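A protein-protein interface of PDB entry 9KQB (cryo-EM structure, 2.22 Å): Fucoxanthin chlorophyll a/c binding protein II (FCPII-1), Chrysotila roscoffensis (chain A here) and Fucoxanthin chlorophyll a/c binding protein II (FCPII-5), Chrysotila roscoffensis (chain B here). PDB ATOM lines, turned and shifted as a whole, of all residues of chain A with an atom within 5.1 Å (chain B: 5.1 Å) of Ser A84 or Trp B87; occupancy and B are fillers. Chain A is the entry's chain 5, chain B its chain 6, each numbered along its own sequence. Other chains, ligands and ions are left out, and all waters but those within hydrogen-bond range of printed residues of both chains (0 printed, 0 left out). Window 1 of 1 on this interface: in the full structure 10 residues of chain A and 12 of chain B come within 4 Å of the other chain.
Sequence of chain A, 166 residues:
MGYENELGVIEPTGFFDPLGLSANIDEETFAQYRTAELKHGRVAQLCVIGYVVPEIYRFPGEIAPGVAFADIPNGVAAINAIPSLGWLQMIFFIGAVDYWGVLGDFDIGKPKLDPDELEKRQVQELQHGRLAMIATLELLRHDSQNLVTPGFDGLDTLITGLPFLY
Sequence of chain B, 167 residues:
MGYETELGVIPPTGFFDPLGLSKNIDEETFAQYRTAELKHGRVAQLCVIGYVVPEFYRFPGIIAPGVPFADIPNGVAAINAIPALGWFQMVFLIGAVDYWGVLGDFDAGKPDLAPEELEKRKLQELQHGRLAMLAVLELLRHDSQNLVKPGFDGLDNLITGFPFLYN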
ATOM      1  N   ILE A  82     -20.413 -19.935  -3.033  1.00  0.00           N
ATOM      2  CA  ILE A  82     -20.008 -19.642  -1.661  1.00  0.00           C
ATOM      3  C   ILE A  82     -18.553 -19.187  -1.700  1.00  0.00           C
ATOM      4  O   ILE A  82     -17.753 -19.775  -2.444  1.00  0.00           O
ATOM      5  CB  ILE A  82     -20.208 -20.864  -0.747  1.00  0.00           C
ATOM      6  CG1 ILE A  82     -21.694 -21.212  -0.639  1.00  0.00           C
ATOM      7  CG2 ILE A  82     -19.629 -20.627   0.642  1.00  0.00           C
ATOM      8  CD1 ILE A  82     -21.981 -22.693  -0.660  1.00  0.00           C
ATOM      9  N   PRO A  83     -18.183 -18.125  -0.977  1.00  0.00           N
ATOM     10  CA  PRO A  83     -16.776 -17.709  -0.927  1.00  0.00           C
ATOM     11  C   PRO A  83     -15.886 -18.806  -0.360  1.00  0.00           C
ATOM     12  O   PRO A  83     -16.303 -19.588   0.497  1.00  0.00           O
ATOM     13  CB  PRO A  83     -16.805 -16.480  -0.012  1.00  0.00           C
ATOM     14  CG  PRO A  83     -18.181 -15.939  -0.165  1.00  0.00           C
ATOM     15  CD  PRO A  83     -19.072 -17.135  -0.345  1.00  0.00           C
ATOM     16  N   SER A  84     -14.652 -18.867  -0.874  1.00  0.00           N
ATOM     17  CA  SER A  84     -13.729 -19.927  -0.475  1.00  0.00           C
ATOM     18  C   SER A  84     -13.353 -19.810   0.996  1.00  0.00           C
ATOM     19  O   SER A  84     -13.204 -20.827   1.680  1.00  0.00           O
ATOM     20  CB  SER A  84     -12.483 -19.909  -1.360  1.00  0.00           C
ATOM     21  OG  SER A  84     -12.833 -19.755  -2.724  1.00  0.00           O
ATOM     22  N   LEU A  85     -13.202 -18.580   1.497  1.00  0.00           N
ATOM     23  CA  LEU A  85     -13.025 -18.364   2.931  1.00  0.00           C
ATOM     24  C   LEU A  85     -14.264 -18.822   3.692  1.00  0.00           C
ATOM     25  O   LEU A  85     -14.169 -19.408   4.778  1.00  0.00           O
ATOM     26  CB  LEU A  85     -12.722 -16.883   3.189  1.00  0.00           C
ATOM     27  CG  LEU A  85     -12.514 -16.287   4.591  1.00  0.00           C
ATOM     28  CD1 LEU A  85     -13.826 -15.839   5.263  1.00  0.00           C
ATOM     29  CD2 LEU A  85     -11.739 -17.248   5.494  1.00  0.00           C
ATOM     30  N   GLY A  86     -15.440 -18.566   3.120  1.00  0.00           N
ATOM     31  CA  GLY A  86     -16.671 -19.010   3.750  1.00  0.00           C
ATOM     32  C   GLY A  86     -16.832 -20.515   3.713  1.00  0.00           C
ATOM     33  O   GLY A  86     -17.597 -21.090   4.487  1.00  0.00           O
ATOM     34  N   TRP A  87     -16.129 -21.173   2.791  1.00  0.00           N
ATOM     35  CA  TRP A  87     -16.154 -22.630   2.754  1.00  0.00           C
ATOM     36  C   TRP A  87     -15.228 -23.229   3.803  1.00  0.00           C
ATOM     37  O   TRP A  87     -15.489 -24.325   4.312  1.00  0.00           O
ATOM     38  CB  TRP A  87     -15.766 -23.123   1.364  1.00  0.00           C
ATOM     39  CG  TRP A  87     -16.909 -23.629   0.544  1.00  0.00           C
ATOM     40  CD1 TRP A  87     -17.396 -23.078  -0.602  1.00  0.00           C
ATOM     41  CD2 TRP A  87     -17.694 -24.803   0.792  1.00  0.00           C
ATOM     42  NE1 TRP A  87     -18.439 -23.830  -1.083  1.00  0.00           N
ATOM     43  CE2 TRP A  87     -18.639 -24.897  -0.248  1.00  0.00           C
ATOM     44  CE3 TRP A  87     -17.686 -25.786   1.786  1.00  0.00           C
ATOM     45  CZ2 TRP A  87     -19.571 -25.928  -0.319  1.00  0.00           C
ATOM     46  CZ3 TRP A  87     -18.614 -26.813   1.713  1.00  0.00           C
ATOM     47  CH2 TRP A  87     -19.544 -26.874   0.669  1.00  0.00           C
ATOM     48  N   LEU A  88     -14.142 -22.524   4.145  1.00  0.00           N
ATOM     49  CA  LEU A  88     -13.101 -23.138   4.967  1.00  0.00           C
ATOM     50  C   LEU A  88     -13.535 -23.342   6.413  1.00  0.00           C
ATOM     51  O   LEU A  88     -13.140 -24.336   7.035  1.00  0.00           O
ATOM     52  CB  LEU A  88     -11.802 -22.329   4.919  1.00  0.00           C
ATOM     53  CG  LEU A  88     -10.957 -22.415   3.645  1.00  0.00           C
ATOM     54  CD1 LEU A  88     -10.384 -21.067   3.291  1.00  0.00           C
ATOM     55  CD2 LEU A  88      -9.842 -23.445   3.794  1.00  0.00           C
ATOM     56  N   ALA B  78      -6.101 -13.561  -1.433  1.00  0.00           N
ATOM     57  CA  ALA B  78      -5.822 -14.770  -2.199  1.00  0.00           C
ATOM     58  C   ALA B  78      -6.728 -15.923  -1.799  1.00  0.00           C
ATOM     59  O   ALA B  78      -6.881 -16.874  -2.575  1.00  0.00           O
ATOM     60  CB  ALA B  78      -4.366 -15.193  -2.013  1.00  0.00           C
ATOM     61  N   ILE B  79      -7.303 -15.869  -0.596  1.00  0.00           N
ATOM     62  CA  ILE B  79      -8.191 -16.932  -0.139  1.00  0.00           C
ATOM     63  C   ILE B  79      -9.450 -16.982  -0.994  1.00  0.00           C
ATOM     64  O   ILE B  79      -9.858 -18.051  -1.460  1.00  0.00           O
ATOM     65  CB  ILE B  79      -8.519 -16.743   1.353  1.00  0.00           C
ATOM     66  CG1 ILE B  79      -7.231 -16.761   2.180  1.00  0.00           C
ATOM     67  CG2 ILE B  79      -9.455 -17.827   1.824  1.00  0.00           C
ATOM     68  CD1 ILE B  79      -7.453 -16.589   3.667  1.00  0.00           C
ATOM     69  N   ASN B  80     -10.068 -15.828  -1.237  1.00  0.00           N
ATOM     70  CA  ASN B  80     -11.262 -15.763  -2.068  1.00  0.00           C
ATOM     71  C   ASN B  80     -10.956 -15.727  -3.559  1.00  0.00           C
ATOM     72  O   ASN B  80     -11.858 -15.984  -4.364  1.00  0.00           O
ATOM     73  CB  ASN B  80     -12.100 -14.537  -1.692  1.00  0.00           C
ATOM     74  CG  ASN B  80     -12.353 -14.440  -0.200  1.00  0.00           C
ATOM     75  OD1 ASN B  80     -13.214 -15.133   0.341  1.00  0.00           O
ATOM     76  ND2 ASN B  80     -11.599 -13.578   0.473  1.00  0.00           N
ATOM     77  N   ILE B  82      -8.660 -17.711  -5.233  1.00  0.00           N
ATOM     78  CA  ILE B  82      -8.632 -19.120  -5.637  1.00  0.00           C
ATOM     79  C   ILE B  82      -9.985 -19.747  -5.315  1.00  0.00           C
ATOM     80  O   ILE B  82     -10.522 -19.513  -4.218  1.00  0.00           O
ATOM     81  CB  ILE B  82      -7.498 -19.848  -4.918  1.00  0.00           C
ATOM     82  CG1 ILE B  82      -6.170 -19.145  -5.194  1.00  0.00           C
ATOM     83  CG2 ILE B  82      -7.426 -21.308  -5.344  1.00  0.00           C
ATOM     84  CD1 ILE B  82      -4.991 -19.811  -4.550  1.00  0.00           C
ATOM     85  N   PRO B  83     -10.586 -20.513  -6.229  1.00  0.00           N
ATOM     86  CA  PRO B  83     -11.886 -21.129  -5.938  1.00  0.00           C
ATOM     87  C   PRO B  83     -11.795 -22.156  -4.820  1.00  0.00           C
ATOM     88  O   PRO B  83     -10.730 -22.702  -4.520  1.00  0.00           O
ATOM     89  CB  PRO B  83     -12.276 -21.783  -7.269  1.00  0.00           C
ATOM     90  CG  PRO B  83     -11.506 -21.031  -8.299  1.00  0.00           C
ATOM     91  CD  PRO B  83     -10.207 -20.673  -7.642  1.00  0.00           C
ATOM     92  N   ALA B  84     -12.948 -22.400  -4.190  1.00  0.00           N
ATOM     93  CA  ALA B  84     -12.996 -23.238  -2.994  1.00  0.00           C
ATOM     94  C   ALA B  84     -12.651 -24.690  -3.298  1.00  0.00           C
ATOM     95  O   ALA B  84     -12.048 -25.373  -2.464  1.00  0.00           O
ATOM     96  CB  ALA B  84     -14.375 -23.143  -2.347  1.00  0.00           C
ATOM     97  N   LEU B  85     -13.041 -25.186  -4.476  1.00  0.00           N
ATOM     98  CA  LEU B  85     -12.694 -26.554  -4.852  1.00  0.00           C
ATOM     99  C   LEU B  85     -11.187 -26.698  -5.026  1.00  0.00           C
ATOM    100  O   LEU B  85     -10.616 -27.765  -4.770  1.00  0.00           O
ATOM    101  CB  LEU B  85     -13.440 -26.957  -6.124  1.00  0.00           C
ATOM    102  CG  LEU B  85     -13.180 -28.348  -6.707  1.00  0.00           C
ATOM    103  CD1 LEU B  85     -13.781 -29.425  -5.820  1.00  0.00           C
ATOM    104  CD2 LEU B  85     -13.720 -28.453  -8.123  1.00  0.00           C
ATOM    105  N   GLY B  86     -10.524 -25.623  -5.453  1.00  0.00           N
ATOM    106  CA  GLY B  86      -9.071 -25.606  -5.427  1.00  0.00           C
ATOM    107  C   GLY B  86      -8.531 -25.657  -4.014  1.00  0.00           C
ATOM    108  O   GLY B  86      -7.504 -26.285  -3.747  1.00  0.00           O
ATOM    109  N   TRP B  87      -9.223 -24.996  -3.082  1.00  0.00           N
ATOM    110  CA  TRP B  87      -8.815 -25.038  -1.681  1.00  0.00           C
ATOM    111  C   TRP B  87      -9.089 -26.404  -1.068  1.00  0.00           C
ATOM    112  O   TRP B  87      -8.367 -26.845  -0.171  1.00  0.00           O
ATOM    113  CB  TRP B  87      -9.518 -23.941  -0.883  1.00  0.00           C
ATOM    114  CG  TRP B  87      -8.906 -22.600  -1.066  1.00  0.00           C
ATOM    115  CD1 TRP B  87      -9.312 -21.621  -1.922  1.00  0.00           C
ATOM    116  CD2 TRP B  87      -7.747 -22.095  -0.397  1.00  0.00           C
ATOM    117  NE1 TRP B  87      -8.488 -20.528  -1.811  1.00  0.00           N
ATOM    118  CE2 TRP B  87      -7.515 -20.797  -0.886  1.00  0.00           C
ATOM    119  CE3 TRP B  87      -6.885 -22.614   0.574  1.00  0.00           C
ATOM    120  CZ2 TRP B  87      -6.457 -20.011  -0.439  1.00  0.00           C
ATOM    121  CZ3 TRP B  87      -5.836 -21.831   1.017  1.00  0.00           C
ATOM    122  CH2 TRP B  87      -5.633 -20.542   0.511  1.00  0.00           C
ATOM    123  N   PHE B  88     -10.144 -27.083  -1.533  1.00  0.00           N
ATOM    124  CA  PHE B  88     -10.477 -28.407  -1.014  1.00  0.00           C
ATOM    125  C   PHE B  88      -9.370 -29.407  -1.312  1.00  0.00           C
ATOM    126  O   PHE B  88      -9.021 -30.239  -0.468  1.00  0.00           O
ATOM    127  CB  PHE B  88     -11.796 -28.902  -1.611  1.00  0.00           C
ATOM    128  CG  PHE B  88     -12.998 -28.097  -1.213  1.00  0.00           C
ATOM    129  CD1 PHE B  88     -12.931 -27.260  -0.113  1.00  0.00           C
ATOM    130  CD2 PHE B  88     -14.175 -28.143  -1.946  1.00  0.00           C
ATOM    131  CE1 PHE B  88     -14.018 -26.512   0.267  1.00  0.00           C
ATOM    132  CE2 PHE B  88     -15.268 -27.394  -1.568  1.00  0.00           C
ATOM    133  CZ  PHE B  88     -15.184 -26.578  -0.459  1.00  0.00           C
ATOM    134  N   GLN B  89      -8.815 -29.344  -2.524  1.00  0.00           N
ATOM    135  CA  GLN B  89      -7.725 -30.233  -2.904  1.00  0.00           C
ATOM    136  C   GLN B  89      -6.472 -29.942  -2.084  1.00  0.00           C
ATOM    137  O   GLN B  89      -5.790 -30.862  -1.618  1.00  0.00           O
ATOM    138  CB  GLN B  89      -7.448 -30.090  -4.400  1.00  0.00           C
ATOM    139  CG  GLN B  89      -8.411 -30.864  -5.282  1.00  0.00           C
ATOM    140  CD  GLN B  89      -8.775 -30.112  -6.546  1.00  0.00           C
ATOM    141  OE1 GLN B  89      -8.719 -30.658  -7.647  1.00  0.00           O
ATOM    142  NE2 GLN B  89      -9.154 -28.851  -6.393  1.00  0.00           N
ATOM    143  N   MET B  90      -6.165 -28.656  -1.887  1.00  0.00           N
ATOM    144  CA  MET B  90      -4.972 -28.278  -1.133  1.00  0.00           C
ATOM    145  C   MET B  90      -5.097 -28.633   0.342  1.00  0.00           C
ATOM    146  O   MET B  90      -4.151 -29.157   0.941  1.00  0.00           O
ATOM    147  CB  MET B  90      -4.701 -26.780  -1.292  1.00  0.00           C
ATOM    148  CG  MET B  90      -4.411 -26.336  -2.715  1.00  0.00           C
ATOM    149  SD  MET B  90      -4.074 -24.568  -2.877  1.00  0.00           S
ATOM    150  CE  MET B  90      -3.531 -24.139  -1.224  1.00  0.00           C
ATOM    151  N   VAL B  91      -6.256 -28.348   0.945  1.00  0.00           N
ATOM    152  CA  VAL B  91      -6.457 -28.616   2.367  1.00  0.00           C
ATOM    153  C   VAL B  91      -6.420 -30.116   2.642  1.00  0.00           C
ATOM    154  O   VAL B  91      -5.795 -30.571   3.609  1.00  0.00           O
ATOM    155  CB  VAL B  91      -7.773 -27.970   2.844  1.00  0.00           C
ATOM    156  CG1 VAL B  91      -8.220 -28.538   4.175  1.00  0.00           C
ATOM    157  CG2 VAL B  91      -7.624 -26.457   2.945  1.00  0.00           C
ATOM    158  N   PHE B  92      -7.061 -30.911   1.780  1.00  0.00           N
ATOM    159  CA  PHE B  92      -7.095 -32.357   1.980  1.00  0.00           C
ATOM    160  C   PHE B  92      -5.726 -32.999   1.773  1.00  0.00           C
ATOM    161  O   PHE B  92      -5.377 -33.940   2.496  1.00  0.00           O
ATOM    162  CB  PHE B  92      -8.131 -32.987   1.050  1.00  0.00           C
ATOM    163  CG  PHE B  92      -9.482 -33.160   1.683  1.00  0.00           C
ATOM    164  CD1 PHE B  92      -9.621 -33.872   2.864  1.00  0.00           C
ATOM    165  CD2 PHE B  92     -10.611 -32.606   1.101  1.00  0.00           C
ATOM    166  CE1 PHE B  92     -10.862 -34.032   3.451  1.00  0.00           C
ATOM    167  CE2 PHE B  92     -11.856 -32.762   1.684  1.00  0.00           C
ATOM    168  CZ  PHE B  92     -11.982 -33.476   2.859  1.00  0.00           C
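The backbone carbonyl oxygen (O) of Ile B82 lies within hydrogen-bond range of the side-chain hydroxyl (OG) of Ser A84, 2.8 Å away.
The side-chain hydroxyl (OG) of Ser A84 is in hydrogen-bond range of the backbone NH (N) of Ala B84.
O of Ile B79 is in hydrogen-bond range of NE1 of Trp B87, at 2.9 Å.
The backbone carbonyl oxygen (O) of Ile B82 lies within hydrogen-bond range of the indole nitrogen (NE1) of Trp B87, at 3.3 Å.
Asn B80 touches Pro A83.
O of Ile B79 touches CB of Ser A84, 3.2 Å away.
Ser A84 touches Pro B83.
Trp B87 touches Ser A84.
Leu A85 touches Ile B79.
OD1 of Asn B80 touches CB of Leu A85 (3.4 Å).
Trp A87 touches Ala B84.
Phe B88 touches Trp A87 (CZ to CD2, 3.3 Å).
Ile B79 touches Leu A88.
Val B91 touches Leu A88 (CG2 to CD2, 3.8 Å).
Of chain B, only Ile B79, Ile B82, Pro B83, Ala B84 and Trp B87 come within 4 Å of Ser A84.
Of chain A, only Ser A84 (3.6 Å) comes within 4 Å of Trp B87.
Of the printed residues of chain A, Ala B84 touches Ser A84 (3.0 Å) and Trp A87 (3.5 Å).
Printed residues of chain B within 4 Å of Pro A83: Asn B80.
Of the printed residues of chain B, Trp A87 touches Ala B84 (3.5 Å) and Phe B88 (3.3 Å).
Of the printed residues of chain A, Ile B79 touches Ser A84 (3.2 Å), Leu A85 (3.7 Å) and Leu A88 (3.7 Å).
Gly A86 touches none of the printed residues of chain B.
Ile A82 touches none of the printed residues of chain B.
The nearest residue of chain B that does not touch Ser A84 is Asn B80 (4.2 Å).
The nearest printed residue of chain A that does not touch Phe B88 is Leu A88 (5.6 Å).
Of the 14 printed residues of chain B, 8 touch a printed residue of chain A.
Printed residues of chain B that touch a printed residue of chain A: Ile B79, Asn B80, Ile B82, Pro B83, Ala B84, Trp B87, Phe B88 and Val B91.
Hydrophobic or aromatic side chains of chain B that line the printed part of chain A: Ile B79, Ala B84, Trp B87, Phe B88 and Val B91.
Among the printed residues, 12 pairs touch across the chains.
Among the printed residues, no Asp or Glu carboxylate lies within 4 Å of a Lys or Arg side-chain nitrogen of the other chain.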
